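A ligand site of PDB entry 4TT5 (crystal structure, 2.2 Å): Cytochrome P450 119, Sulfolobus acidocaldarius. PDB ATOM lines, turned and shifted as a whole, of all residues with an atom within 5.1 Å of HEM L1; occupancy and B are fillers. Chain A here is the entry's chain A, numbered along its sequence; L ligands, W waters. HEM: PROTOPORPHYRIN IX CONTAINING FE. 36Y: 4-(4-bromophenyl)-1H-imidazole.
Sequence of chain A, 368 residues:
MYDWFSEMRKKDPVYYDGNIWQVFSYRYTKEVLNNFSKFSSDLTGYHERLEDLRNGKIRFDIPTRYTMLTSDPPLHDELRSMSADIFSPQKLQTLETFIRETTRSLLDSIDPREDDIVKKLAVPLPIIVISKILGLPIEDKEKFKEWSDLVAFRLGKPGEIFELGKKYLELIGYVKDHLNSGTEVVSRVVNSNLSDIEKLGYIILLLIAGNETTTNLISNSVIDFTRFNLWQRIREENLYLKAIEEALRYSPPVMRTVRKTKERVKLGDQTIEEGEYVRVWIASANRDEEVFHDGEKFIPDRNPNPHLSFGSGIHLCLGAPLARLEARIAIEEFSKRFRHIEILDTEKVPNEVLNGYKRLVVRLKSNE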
ATOM      1  N   LEU A  33      16.975 -12.263 -12.934  1.00  0.00           N
ATOM      2  CA  LEU A  33      16.271 -11.012 -13.244  1.00  0.00           C
ATOM      3  C   LEU A  33      14.889 -10.947 -12.598  1.00  0.00           C
ATOM      4  O   LEU A  33      14.466  -9.900 -12.123  1.00  0.00           O
ATOM      5  CB  LEU A  33      16.160 -10.819 -14.757  1.00  0.00           C
ATOM      6  CG  LEU A  33      17.518 -10.610 -15.462  1.00  0.00           C
ATOM      7  CD1 LEU A  33      17.359 -10.558 -16.973  1.00  0.00           C
ATOM      8  CD2 LEU A  33      18.232  -9.353 -14.940  1.00  0.00           C
ATOM      9  N   SER A  41      18.642  -4.947  -7.055  1.00  0.00           N
ATOM     10  CA  SER A  41      19.190  -3.919  -7.956  1.00  0.00           C
ATOM     11  C   SER A  41      19.703  -2.713  -7.189  1.00  0.00           C
ATOM     12  O   SER A  41      20.265  -1.774  -7.757  1.00  0.00           O
ATOM     13  CB  SER A  41      18.141  -3.458  -8.978  1.00  0.00           C
ATOM     14  OG  SER A  41      17.797  -4.505  -9.871  1.00  0.00           O
ATOM     15  N   MET A  68      15.083   4.652 -10.510  1.00  0.00           N
ATOM     16  CA  MET A  68      14.390   3.379 -10.475  1.00  0.00           C
ATOM     17  C   MET A  68      15.296   2.210 -10.885  1.00  0.00           C
ATOM     18  O   MET A  68      15.071   1.070 -10.492  1.00  0.00           O
ATOM     19  CB  MET A  68      13.159   3.405 -11.382  1.00  0.00           C
ATOM     20  CG  MET A  68      13.499   3.500 -12.889  1.00  0.00           C
ATOM     21  SD  MET A  68      12.010   3.534 -13.940  1.00  0.00           S
ATOM     22  CE  MET A  68      11.596   5.263 -13.766  1.00  0.00           C
ATOM     23  N   LEU A  69      16.323   2.488 -11.685  1.00  0.00           N
ATOM     24  CA  LEU A  69      17.224   1.448 -12.188  1.00  0.00           C
ATOM     25  C   LEU A  69      17.965   0.751 -11.045  1.00  0.00           C
ATOM     26  O   LEU A  69      18.199  -0.461 -11.091  1.00  0.00           O
ATOM     27  CB  LEU A  69      18.246   2.053 -13.175  1.00  0.00           C
ATOM     28  CG  LEU A  69      19.220   1.097 -13.841  1.00  0.00           C
ATOM     29  CD1 LEU A  69      18.487   0.112 -14.771  1.00  0.00           C
ATOM     30  CD2 LEU A  69      20.290   1.870 -14.607  1.00  0.00           C
ATOM     31  N   HIS A  76      11.020   1.189  -6.156  1.00  0.00           N
ATOM     32  CA  HIS A  76      11.126   1.032  -7.603  1.00  0.00           C
ATOM     33  C   HIS A  76       9.792   1.250  -8.304  1.00  0.00           C
ATOM     34  O   HIS A  76       9.714   1.983  -9.281  1.00  0.00           O
ATOM     35  CB  HIS A  76      11.627  -0.356  -8.013  1.00  0.00           C
ATOM     36  CG  HIS A  76      11.391  -0.659  -9.454  1.00  0.00           C
ATOM     37  ND1 HIS A  76      10.232  -1.253  -9.916  1.00  0.00           N
ATOM     38  CD2 HIS A  76      12.140  -0.368 -10.559  1.00  0.00           C
ATOM     39  CE1 HIS A  76      10.306  -1.362 -11.244  1.00  0.00           C
ATOM     40  NE2 HIS A  76      11.441  -0.846 -11.654  1.00  0.00           N
ATOM     41  N   ARG A  80       8.614   4.251 -10.902  1.00  0.00           N
ATOM     42  CA  ARG A  80       8.343   3.969 -12.307  1.00  0.00           C
ATOM     43  C   ARG A  80       6.909   4.328 -12.667  1.00  0.00           C
ATOM     44  O   ARG A  80       6.637   4.727 -13.788  1.00  0.00           O
ATOM     45  CB  ARG A  80       8.633   2.500 -12.611  1.00  0.00           C
ATOM     46  CG  ARG A  80       8.289   2.112 -14.030  1.00  0.00           C
ATOM     47  CD  ARG A  80       9.028   0.889 -14.464  1.00  0.00           C
ATOM     48  NE  ARG A  80       8.479   0.336 -15.695  1.00  0.00           N
ATOM     49  CZ  ARG A  80       9.134  -0.489 -16.496  1.00  0.00           C
ATOM     50  NH1 ARG A  80      10.393  -0.819 -16.217  1.00  0.00           N
ATOM     51  NH2 ARG A  80       8.544  -0.957 -17.585  1.00  0.00           N
ATOM     52  N   PHE A  87       5.419   5.817 -21.719  1.00  0.00           N
ATOM     53  CA  PHE A  87       6.278   4.943 -22.489  1.00  0.00           C
ATOM     54  C   PHE A  87       5.592   3.643 -22.872  1.00  0.00           C
ATOM     55  O   PHE A  87       6.249   2.711 -23.311  1.00  0.00           O
ATOM     56  CB  PHE A  87       7.560   4.649 -21.705  1.00  0.00           C
ATOM     57  CG  PHE A  87       8.460   5.847 -21.599  1.00  0.00           C
ATOM     58  CD1 PHE A  87       9.355   6.149 -22.629  1.00  0.00           C
ATOM     59  CD2 PHE A  87       8.401   6.677 -20.483  1.00  0.00           C
ATOM     60  CE1 PHE A  87      10.167   7.268 -22.555  1.00  0.00           C
ATOM     61  CE2 PHE A  87       9.229   7.789 -20.401  1.00  0.00           C
ATOM     62  CZ  PHE A  87      10.114   8.081 -21.441  1.00  0.00           C
ATOM     63  N   ILE A 130      13.401  11.793 -27.921  1.00  0.00           N
ATOM     64  CA  ILE A 130      13.282  11.883 -26.479  1.00  0.00           C
ATOM     65  C   ILE A 130      13.120  13.343 -26.082  1.00  0.00           C
ATOM     66  O   ILE A 130      12.373  13.654 -25.167  1.00  0.00           O
ATOM     67  CB  ILE A 130      14.489  11.241 -25.711  1.00  0.00           C
ATOM     68  CG1 ILE A 130      14.158  11.125 -24.214  1.00  0.00           C
ATOM     69  CG2 ILE A 130      15.768  12.053 -25.891  1.00  0.00           C
ATOM     70  CD1 ILE A 130      12.960  10.262 -23.934  1.00  0.00           C
ATOM     71  N   LEU A 205      18.010  10.288 -16.291  1.00  0.00           N
ATOM     72  CA  LEU A 205      17.813   8.923 -16.757  1.00  0.00           C
ATOM     73  C   LEU A 205      16.920   8.885 -18.006  1.00  0.00           C
ATOM     74  O   LEU A 205      17.257   8.254 -19.011  1.00  0.00           O
ATOM     75  CB  LEU A 205      17.201   8.082 -15.635  1.00  0.00           C
ATOM     76  CG  LEU A 205      17.065   6.581 -15.891  1.00  0.00           C
ATOM     77  CD1 LEU A 205      18.417   5.884 -15.777  1.00  0.00           C
ATOM     78  CD2 LEU A 205      16.055   5.988 -14.919  1.00  0.00           C
ATOM     79  N   LEU A 206      15.771   9.553 -17.959  1.00  0.00           N
ATOM     80  CA  LEU A 206      14.867   9.509 -19.102  1.00  0.00           C
ATOM     81  C   LEU A 206      15.475  10.225 -20.313  1.00  0.00           C
ATOM     82  O   LEU A 206      15.356   9.743 -21.434  1.00  0.00           O
ATOM     83  CB  LEU A 206      13.507  10.130 -18.744  1.00  0.00           C
ATOM     84  CG  LEU A 206      12.698   9.439 -17.633  1.00  0.00           C
ATOM     85  CD1 LEU A 206      11.305  10.033 -17.483  1.00  0.00           C
ATOM     86  CD2 LEU A 206      12.596   7.962 -17.868  1.00  0.00           C
ATOM     87  N   GLY A 210      18.815   6.377 -22.518  1.00  0.00           N
ATOM     88  CA  GLY A 210      18.358   5.545 -23.619  1.00  0.00           C
ATOM     89  C   GLY A 210      18.882   5.886 -25.009  1.00  0.00           C
ATOM     90  O   GLY A 210      18.592   5.173 -25.968  1.00  0.00           O
ATOM     91  N   THR A 213      21.892   3.375 -26.441  1.00  0.00           N
ATOM     92  CA  THR A 213      21.411   2.004 -26.605  1.00  0.00           C
ATOM     93  C   THR A 213      20.526   1.894 -27.837  1.00  0.00           C
ATOM     94  O   THR A 213      20.595   0.915 -28.588  1.00  0.00           O
ATOM     95  CB  THR A 213      20.620   1.490 -25.371  1.00  0.00           C
ATOM     96  OG1 THR A 213      19.639   2.460 -24.997  1.00  0.00           O
ATOM     97  CG2 THR A 213      21.566   1.273 -24.171  1.00  0.00           C
ATOM     98  N   THR A 214      19.688   2.902 -28.060  1.00  0.00           N
ATOM     99  CA  THR A 214      18.809   2.899 -29.217  1.00  0.00           C
ATOM    100  C   THR A 214      19.610   3.132 -30.510  1.00  0.00           C
ATOM    101  O   THR A 214      19.377   2.495 -31.538  1.00  0.00           O
ATOM    102  CB  THR A 214      17.687   3.967 -29.092  1.00  0.00           C
ATOM    103  OG1 THR A 214      16.973   3.767 -27.871  1.00  0.00           O
ATOM    104  CG2 THR A 214      16.709   3.878 -30.246  1.00  0.00           C
ATOM    105  N   LEU A 217      21.121  -0.180 -31.367  1.00  0.00           N
ATOM    106  CA  LEU A 217      20.181  -1.103 -32.019  1.00  0.00           C
ATOM    107  C   LEU A 217      20.063  -0.815 -33.514  1.00  0.00           C
ATOM    108  O   LEU A 217      20.033  -1.732 -34.329  1.00  0.00           O
ATOM    109  CB  LEU A 217      18.790  -1.035 -31.378  1.00  0.00           C
ATOM    110  CG  LEU A 217      17.654  -1.833 -32.041  1.00  0.00           C
ATOM    111  CD1 LEU A 217      17.997  -3.296 -32.238  1.00  0.00           C
ATOM    112  CD2 LEU A 217      16.334  -1.719 -31.248  1.00  0.00           C
ATOM    113  N   LEU A 248      17.926  -7.628 -31.994  1.00  0.00           N
ATOM    114  CA  LEU A 248      17.989  -7.459 -30.536  1.00  0.00           C
ATOM    115  C   LEU A 248      18.586  -8.694 -29.904  1.00  0.00           C
ATOM    116  O   LEU A 248      19.476  -8.588 -29.068  1.00  0.00           O
ATOM    117  CB  LEU A 248      16.609  -7.179 -29.932  1.00  0.00           C
ATOM    118  CG  LEU A 248      16.143  -5.722 -30.006  1.00  0.00           C
ATOM    119  CD1 LEU A 248      14.635  -5.625 -29.981  1.00  0.00           C
ATOM    120  CD2 LEU A 248      16.781  -4.925 -28.865  1.00  0.00           C
ATOM    121  N   PRO A 253      22.324  -4.456 -27.661  1.00  0.00           N
ATOM    122  CA  PRO A 253      23.000  -3.189 -27.285  1.00  0.00           C
ATOM    123  C   PRO A 253      23.516  -3.184 -25.833  1.00  0.00           C
ATOM    124  O   PRO A 253      24.505  -2.523 -25.542  1.00  0.00           O
ATOM    125  CB  PRO A 253      21.895  -2.146 -27.482  1.00  0.00           C
ATOM    126  CG  PRO A 253      20.988  -2.764 -28.568  1.00  0.00           C
ATOM    127  CD  PRO A 253      20.990  -4.233 -28.246  1.00  0.00           C
ATOM    128  N   VAL A 254      22.856  -3.919 -24.946  1.00  0.00           N
ATOM    129  CA  VAL A 254      23.316  -4.065 -23.572  1.00  0.00           C
ATOM    130  C   VAL A 254      23.673  -5.534 -23.372  1.00  0.00           C
ATOM    131  O   VAL A 254      22.787  -6.399 -23.404  1.00  0.00           O
ATOM    132  CB  VAL A 254      22.272  -3.600 -22.549  1.00  0.00           C
ATOM    133  CG1 VAL A 254      22.827  -3.672 -21.114  1.00  0.00           C
ATOM    134  CG2 VAL A 254      21.830  -2.197 -22.845  1.00  0.00           C
ATOM    135  N   THR A 257      23.815  -7.301 -17.384  1.00  0.00           N
ATOM    136  CA  THR A 257      23.509  -6.447 -16.241  1.00  0.00           C
ATOM    137  C   THR A 257      23.940  -7.170 -14.969  1.00  0.00           C
ATOM    138  O   THR A 257      24.545  -8.249 -15.040  1.00  0.00           O
ATOM    139  CB  THR A 257      22.006  -6.033 -16.206  1.00  0.00           C
ATOM    140  OG1 THR A 257      21.800  -5.067 -15.162  1.00  0.00           O
ATOM    141  CG2 THR A 257      21.113  -7.235 -15.990  1.00  0.00           C
ATOM    142  N   VAL A 258      23.676  -6.580 -13.815  1.00  0.00           N
ATOM    143  CA  VAL A 258      24.226  -7.095 -12.580  1.00  0.00           C
ATOM    144  C   VAL A 258      23.219  -6.968 -11.414  1.00  0.00           C
ATOM    145  O   VAL A 258      22.304  -6.126 -11.444  1.00  0.00           O
ATOM    146  CB  VAL A 258      25.589  -6.390 -12.254  1.00  0.00           C
ATOM    147  CG1 VAL A 258      25.404  -4.897 -12.083  1.00  0.00           C
ATOM    148  CG2 VAL A 258      26.286  -7.045 -11.064  1.00  0.00           C
ATOM    149  N   ARG A 259      23.347  -7.861 -10.429  1.00  0.00           N
ATOM    150  CA  ARG A 259      22.520  -7.867  -9.230  1.00  0.00           C
ATOM    151  C   ARG A 259      23.422  -8.114  -8.015  1.00  0.00           C
ATOM    152  O   ARG A 259      24.590  -8.526  -8.169  1.00  0.00           O
ATOM    153  CB  ARG A 259      21.428  -8.958  -9.324  1.00  0.00           C
ATOM    154  CG  ARG A 259      20.405  -8.782 -10.457  1.00  0.00           C
ATOM    155  CD  ARG A 259      19.520  -7.556 -10.199  1.00  0.00           C
ATOM    156  NE  ARG A 259      18.396  -7.420 -11.131  1.00  0.00           N
ATOM    157  CZ  ARG A 259      18.417  -6.666 -12.230  1.00  0.00           C
ATOM    158  NH1 ARG A 259      19.504  -5.990 -12.540  1.00  0.00           N
ATOM    159  NH2 ARG A 259      17.336  -6.576 -13.007  1.00  0.00           N
ATOM    160  N   ILE A 282      23.302 -11.271 -20.656  1.00  0.00           N
ATOM    161  CA  ILE A 282      22.175 -11.236 -21.570  1.00  0.00           C
ATOM    162  C   ILE A 282      22.553 -11.773 -22.941  1.00  0.00           C
ATOM    163  O   ILE A 282      21.811 -12.553 -23.536  1.00  0.00           O
ATOM    164  CB  ILE A 282      21.647  -9.789 -21.741  1.00  0.00           C
ATOM    165  CG1 ILE A 282      20.946  -9.309 -20.466  1.00  0.00           C
ATOM    166  CG2 ILE A 282      20.724  -9.674 -22.951  1.00  0.00           C
ATOM    167  CD1 ILE A 282      20.749  -7.790 -20.453  1.00  0.00           C
ATOM    168  N   LEU A 308      16.327 -11.652 -23.969  1.00  0.00           N
ATOM    169  CA  LEU A 308      16.411 -10.909 -22.715  1.00  0.00           C
ATOM    170  C   LEU A 308      17.062  -9.535 -22.886  1.00  0.00           C
ATOM    171  O   LEU A 308      17.578  -8.967 -21.920  1.00  0.00           O
ATOM    172  CB  LEU A 308      17.190 -11.738 -21.677  1.00  0.00           C
ATOM    173  CG  LEU A 308      16.604 -13.121 -21.386  1.00  0.00           C
ATOM    174  CD1 LEU A 308      17.380 -13.856 -20.293  1.00  0.00           C
ATOM    175  CD2 LEU A 308      15.110 -13.026 -21.026  1.00  0.00           C
ATOM    176  N   SER A 309      17.011  -8.984 -24.100  1.00  0.00           N
ATOM    177  CA  SER A 309      17.811  -7.792 -24.398  1.00  0.00           C
ATOM    178  C   SER A 309      17.270  -6.518 -23.752  1.00  0.00           C
ATOM    179  O   SER A 309      18.004  -5.546 -23.602  1.00  0.00           O
ATOM    180  CB  SER A 309      17.956  -7.596 -25.914  1.00  0.00           C
ATOM    181  OG  SER A 309      18.598  -8.733 -26.483  1.00  0.00           O
ATOM    182  N   PHE A 310      15.990  -6.543 -23.367  1.00  0.00           N
ATOM    183  CA  PHE A 310      15.399  -5.479 -22.567  1.00  0.00           C
ATOM    184  C   PHE A 310      15.295  -5.880 -21.082  1.00  0.00           C
ATOM    185  O   PHE A 310      14.688  -5.168 -20.276  1.00  0.00           O
ATOM    186  CB  PHE A 310      14.017  -5.110 -23.128  1.00  0.00           C
ATOM    187  CG  PHE A 310      14.067  -4.347 -24.434  1.00  0.00           C
ATOM    188  CD1 PHE A 310      14.735  -3.135 -24.514  1.00  0.00           C
ATOM    189  CD2 PHE A 310      13.442  -4.849 -25.574  1.00  0.00           C
ATOM    190  CE1 PHE A 310      14.768  -2.423 -25.715  1.00  0.00           C
ATOM    191  CE2 PHE A 310      13.476  -4.138 -26.776  1.00  0.00           C
ATOM    192  CZ  PHE A 310      14.147  -2.937 -26.849  1.00  0.00           C
ATOM    193  N   GLY A 311      15.877  -7.019 -20.729  1.00  0.00           N
ATOM    194  CA  GLY A 311      15.806  -7.534 -19.373  1.00  0.00           C
ATOM    195  C   GLY A 311      14.595  -8.449 -19.199  1.00  0.00           C
ATOM    196  O   GLY A 311      14.030  -8.942 -20.173  1.00  0.00           O
ATOM    197  N   ILE A 314      10.540  -6.874 -13.205  1.00  0.00           N
ATOM    198  CA  ILE A 314      10.042  -5.535 -12.861  1.00  0.00           C
ATOM    199  C   ILE A 314      10.890  -4.413 -13.460  1.00  0.00           C
ATOM    200  O   ILE A 314      10.391  -3.296 -13.623  1.00  0.00           O
ATOM    201  CB  ILE A 314       9.953  -5.331 -11.318  1.00  0.00           C
ATOM    202  CG1 ILE A 314      11.338  -5.420 -10.681  1.00  0.00           C
ATOM    203  CG2 ILE A 314       9.033  -6.371 -10.679  1.00  0.00           C
ATOM    204  CD1 ILE A 314      11.337  -4.981  -9.257  1.00  0.00           C
ATOM    205  N   HIS A 315      12.146  -4.690 -13.810  1.00  0.00           N
ATOM    206  CA  HIS A 315      12.983  -3.639 -14.421  1.00  0.00           C
ATOM    207  C   HIS A 315      13.013  -3.689 -15.937  1.00  0.00           C
ATOM    208  O   HIS A 315      13.789  -2.962 -16.572  1.00  0.00           O
ATOM    209  CB  HIS A 315      14.427  -3.705 -13.896  1.00  0.00           C
ATOM    210  CG  HIS A 315      14.554  -3.374 -12.457  1.00  0.00           C
ATOM    211  ND1 HIS A 315      14.668  -2.070 -11.997  1.00  0.00           N
ATOM    212  CD2 HIS A 315      14.605  -4.164 -11.340  1.00  0.00           C
ATOM    213  CE1 HIS A 315      14.781  -2.075 -10.677  1.00  0.00           C
ATOM    214  NE2 HIS A 315      14.746  -3.332 -10.257  1.00  0.00           N
ATOM    215  N   LEU A 316      12.182  -4.566 -16.509  1.00  0.00           N
ATOM    216  CA  LEU A 316      12.067  -4.693 -17.970  1.00  0.00           C
ATOM    217  C   LEU A 316      12.035  -3.302 -18.613  1.00  0.00           C
ATOM    218  O   LEU A 316      11.226  -2.461 -18.210  1.00  0.00           O
ATOM    219  CB  LEU A 316      10.808  -5.478 -18.350  1.00  0.00           C
ATOM    220  CG  LEU A 316      10.567  -5.617 -19.856  1.00  0.00           C
ATOM    221  CD1 LEU A 316      11.443  -6.692 -20.432  1.00  0.00           C
ATOM    222  CD2 LEU A 316       9.080  -5.915 -20.132  1.00  0.00           C
ATOM    223  N   CYS A 317      12.932  -3.073 -19.568  1.00  0.00           N
ATOM    224  CA  CYS A 317      13.243  -1.729 -20.031  1.00  0.00           C
ATOM    225  C   CYS A 317      12.015  -0.842 -20.230  1.00  0.00           C
ATOM    226  O   CYS A 317      11.156  -1.142 -21.047  1.00  0.00           O
ATOM    227  CB  CYS A 317      14.040  -1.768 -21.345  1.00  0.00           C
ATOM    228  SG  CYS A 317      14.346  -0.114 -22.009  1.00  0.00           S
ATOM    229  N   LEU A 318      11.978   0.260 -19.487  1.00  0.00           N
ATOM    230  CA  LEU A 318      10.922   1.263 -19.647  1.00  0.00           C
ATOM    231  C   LEU A 318      10.845   1.790 -21.079  1.00  0.00           C
ATOM    232  O   LEU A 318       9.760   2.128 -21.566  1.00  0.00           O
ATOM    233  CB  LEU A 318      11.144   2.431 -18.681  1.00  0.00           C
ATOM    234  CG  LEU A 318      10.121   3.574 -18.659  1.00  0.00           C
ATOM    235  CD1 LEU A 318       8.720   3.028 -18.340  1.00  0.00           C
ATOM    236  CD2 LEU A 318      10.523   4.672 -17.657  1.00  0.00           C
ATOM    237  N   GLY A 319      11.987   1.880 -21.766  1.00  0.00           N
ATOM    238  CA  GLY A 319      12.001   2.422 -23.107  1.00  0.00           C
ATOM    239  C   GLY A 319      11.836   1.397 -24.225  1.00  0.00           C
ATOM    240  O   GLY A 319      11.964   1.733 -25.398  1.00  0.00           O
ATOM    241  N   ALA A 320      11.564   0.150 -23.872  1.00  0.00           N
ATOM    242  CA  ALA A 320      11.514  -0.895 -24.884  1.00  0.00           C
ATOM    243  C   ALA A 320      10.469  -0.624 -25.993  1.00  0.00           C
ATOM    244  O   ALA A 320      10.789  -0.771 -27.177  1.00  0.00           O
ATOM    245  CB  ALA A 320      11.269  -2.253 -24.241  1.00  0.00           C
ATOM    246  N   LEU A 322       9.380   2.315 -26.979  1.00  0.00           N
ATOM    247  CA  LEU A 322       9.932   3.426 -27.735  1.00  0.00           C
ATOM    248  C   LEU A 322      11.125   2.999 -28.601  1.00  0.00           C
ATOM    249  O   LEU A 322      11.193   3.356 -29.781  1.00  0.00           O
ATOM    250  CB  LEU A 322      10.337   4.560 -26.799  1.00  0.00           C
ATOM    251  CG  LEU A 322      11.020   5.761 -27.457  1.00  0.00           C
ATOM    252  CD1 LEU A 322      10.083   6.395 -28.488  1.00  0.00           C
ATOM    253  CD2 LEU A 322      11.492   6.802 -26.426  1.00  0.00           C
ATOM    254  N   ALA A 323      12.072   2.245 -28.044  1.00  0.00           N
ATOM    255  CA  ALA A 323      13.229   1.778 -28.806  1.00  0.00           C
ATOM    256  C   ALA A 323      12.796   0.905 -29.984  1.00  0.00           C
ATOM    257  O   ALA A 323      13.334   1.024 -31.076  1.00  0.00           O
ATOM    258  CB  ALA A 323      14.205   1.015 -27.906  1.00  0.00           C
HETATM  259  CHA HEM L   1      16.118  -0.672 -18.263  1.00  0.00           C
HETATM  260  CHB HEM L   1      18.085  -2.258 -22.442  1.00  0.00           C
HETATM  261  CHC HEM L   1      16.380   1.736 -24.618  1.00  0.00           C
HETATM  262  CHD HEM L   1      15.257   3.619 -20.295  1.00  0.00           C
HETATM  263  C1A HEM L   1      16.758  -1.465 -19.215  1.00  0.00           C
HETATM  264  C2A HEM L   1      17.299  -2.782 -18.992  1.00  0.00           C
HETATM  265  C3A HEM L   1      17.848  -3.199 -20.137  1.00  0.00           C
HETATM  266  C4A HEM L   1      17.663  -2.165 -21.132  1.00  0.00           C
HETATM  267  CMA HEM L   1      18.545  -4.531 -20.397  1.00  0.00           C
HETATM  268  CAA HEM L   1      17.267  -3.583 -17.660  1.00  0.00           C
HETATM  269  CBA HEM L   1      18.462  -3.259 -16.751  1.00  0.00           C
HETATM  270  CGA HEM L   1      18.331  -4.097 -15.489  1.00  0.00           C
HETATM  271  O1A HEM L   1      17.474  -5.016 -15.413  1.00  0.00           O
HETATM  272  O2A HEM L   1      19.120  -3.858 -14.544  1.00  0.00           O
HETATM  273  C1B HEM L   1      17.739  -1.346 -23.435  1.00  0.00           C
HETATM  274  C2B HEM L   1      17.957  -1.488 -24.854  1.00  0.00           C
HETATM  275  C3B HEM L   1      17.488  -0.368 -25.455  1.00  0.00           C
HETATM  276  C4B HEM L   1      16.971   0.502 -24.423  1.00  0.00           C
HETATM  277  CMB HEM L   1      18.610  -2.733 -25.504  1.00  0.00           C
HETATM  278  CAB HEM L   1      17.436   0.013 -26.955  1.00  0.00           C
HETATM  279  CBB HEM L   1      17.583  -0.867 -27.957  1.00  0.00           C
HETATM  280  C1C HEM L   1      15.917   2.600 -23.648  1.00  0.00           C
HETATM  281  C2C HEM L   1      15.312   3.916 -23.843  1.00  0.00           C
HETATM  282  C3C HEM L   1      15.029   4.414 -22.634  1.00  0.00           C
HETATM  283  C4C HEM L   1      15.422   3.434 -21.649  1.00  0.00           C
HETATM  284  CMC HEM L   1      15.070   4.587 -25.216  1.00  0.00           C
HETATM  285  CAC HEM L   1      14.399   5.762 -22.173  1.00  0.00           C
HETATM  286  CBC HEM L   1      13.831   6.674 -22.953  1.00  0.00           C
HETATM  287  C1D HEM L   1      15.338   2.618 -19.351  1.00  0.00           C
HETATM  288  C2D HEM L   1      14.952   2.731 -17.957  1.00  0.00           C
HETATM  289  C3D HEM L   1      15.190   1.546 -17.382  1.00  0.00           C
HETATM  290  C4D HEM L   1      15.726   0.645 -18.404  1.00  0.00           C
HETATM  291  CMD HEM L   1      14.387   4.035 -17.335  1.00  0.00           C
HETATM  292  CAD HEM L   1      14.920   1.206 -15.901  1.00  0.00           C
HETATM  293  CBD HEM L   1      13.582   0.470 -15.779  1.00  0.00           C
HETATM  294  CGD HEM L   1      13.349   0.043 -14.345  1.00  0.00           C
HETATM  295  O1D HEM L   1      14.315  -0.038 -13.527  1.00  0.00           O
HETATM  296  O2D HEM L   1      12.193  -0.266 -14.005  1.00  0.00           O
HETATM  297  NA  HEM L   1      16.987  -1.129 -20.532  1.00  0.00           N
HETATM  298  NB  HEM L   1      17.151  -0.130 -23.220  1.00  0.00           N
HETATM  299  NC  HEM L   1      15.964   2.345 -22.287  1.00  0.00           N
HETATM  300  ND  HEM L   1      15.811   1.348 -19.573  1.00  0.00           N
HETATM  301 FE   HEM L   1      16.439   0.612 -21.406  1.00  0.00          FE
HETATM  302  C2  36Y L   2      18.633   2.383 -21.195  1.00  0.00           C
HETATM  303  C5  36Y L   2      20.433   1.382 -20.438  1.00  0.00           C
HETATM  304  C4  36Y L   2      19.365   0.476 -20.411  1.00  0.00           C
HETATM  305  C6  36Y L   2      21.879   1.141 -20.030  1.00  0.00           C
HETATM  306  C7  36Y L   2      22.299  -0.024 -19.397  1.00  0.00           C
HETATM  307  C8  36Y L   2      23.653  -0.212 -19.070  1.00  0.00           C
HETATM  308  C9  36Y L   2      24.590   0.772 -19.379  1.00  0.00           C
HETATM  309  C10 36Y L   2      24.154   1.920 -20.020  1.00  0.00           C
HETATM  310 BR   36Y L   2      26.464   0.604 -18.970  1.00  0.00          BR
HETATM  311  C11 36Y L   2      22.814   2.113 -20.345  1.00  0.00           C
HETATM  312  N3  36Y L   2      18.282   1.134 -20.878  1.00  0.00           N
HETATM  313  N1  36Y L   2      19.938   2.540 -20.938  1.00  0.00           N
HETATM  314  O   HOH W   1      17.805  -3.038 -12.175  1.00  0.00           O
HETATM  315  O   HOH W   2      21.664  -2.302 -15.626  1.00  0.00           O
HETATM  316  O   HOH W   3      15.347  -6.703 -16.293  1.00  0.00           O
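SG of Cys 317 binds FE of HEM L1 (2.3 Å).
NE2 of His 76 sits at hydrogen-bond distance from O2D of HEM L1, at 2.5 Å.
A ring nitrogen (ND1) of His 315 sits at hydrogen-bond distance from an oxygen (O1D) of HEM L1 (2.6 Å).
NH2 of Arg 259 is in salt-bridge range of O1A of HEM L1 (2.9 Å).
An oxygen (O2D) of HEM L1 lies within salt-bridge range of the guanidinium group (NH1) of Arg 80 (2.9 Å).
OG1 of Thr 257 is in hydrogen-bond range of O2A of HEM L1, at 3.0 Å.
SG of Cys 317 sits close to N of Gly 319 (3.1 Å).
The side-chain sulfur of Cys 317 lies close to the backbone NH of Ala 320 (3.4 Å).
O of Ile 314 lies close to NE2 of His 76.
A ring nitrogen (NE2) of His 315 is in hydrogen-bond range of the side-chain hydroxyl of Ser 41, at 3.3 Å.
The guanidinium group (NE) of Arg 259 sits at hydrogen-bond distance from the side-chain hydroxyl (OG) of Ser 41.
The backbone carbonyl oxygen (O) of Gly 210 sits at hydrogen-bond distance from the side-chain hydroxyl (OG1) of Thr 213.
OG1 of Thr 214 sits at hydrogen-bond distance from O of Gly 210 (2.9 Å).
O of Leu 248 lies within hydrogen-bond range of OG of Ser 309, 2.7 Å away.
The backbone carbonyl oxygen of Met 68 lies close to an oxygen (O1D) of HEM L1.
Residues that only touch HEM L1: Thr 213 (3.4 Å), Thr 214 (3.4 Å), Ser 309 (3.4 Å), Phe 310 (3.4 Å), Gly 210 (3.5 Å), Ala 323 (3.5 Å), Leu 205 (3.5 Å), Leu 69 (3.5 Å), Ile 314 (3.5 Å), Leu 217 (3.6 Å), Gly 319 (3.7 Å), Gly 311 (3.7 Å), Phe 87 (3.7 Å), Leu 206 (3.7 Å), Val 254 (3.8 Å), Ile 130 (3.8 Å), Leu 318 (3.9 Å), Pro 253 (3.9 Å) and Ile 282 (3.9 Å).
Water W1 lies within hydrogen-bond range of OG of Ser 41 (2.7 Å), O of Leu 69 (2.8 Å), O2A of HEM L1 (2.8 Å), ND1 of His 315 (3.3 Å) and NH1 of Arg 259 (3.4 Å).
Water W2 lies within hydrogen-bond range of the side-chain hydroxyl (OG1) of Thr 257 (2.8 Å) and an oxygen (O2A) of HEM L1 (3.2 Å).
A nitrogen (N3) of 36Y L2 is bound to an iron atom (FE) of HEM L1, at 2.0 Å.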
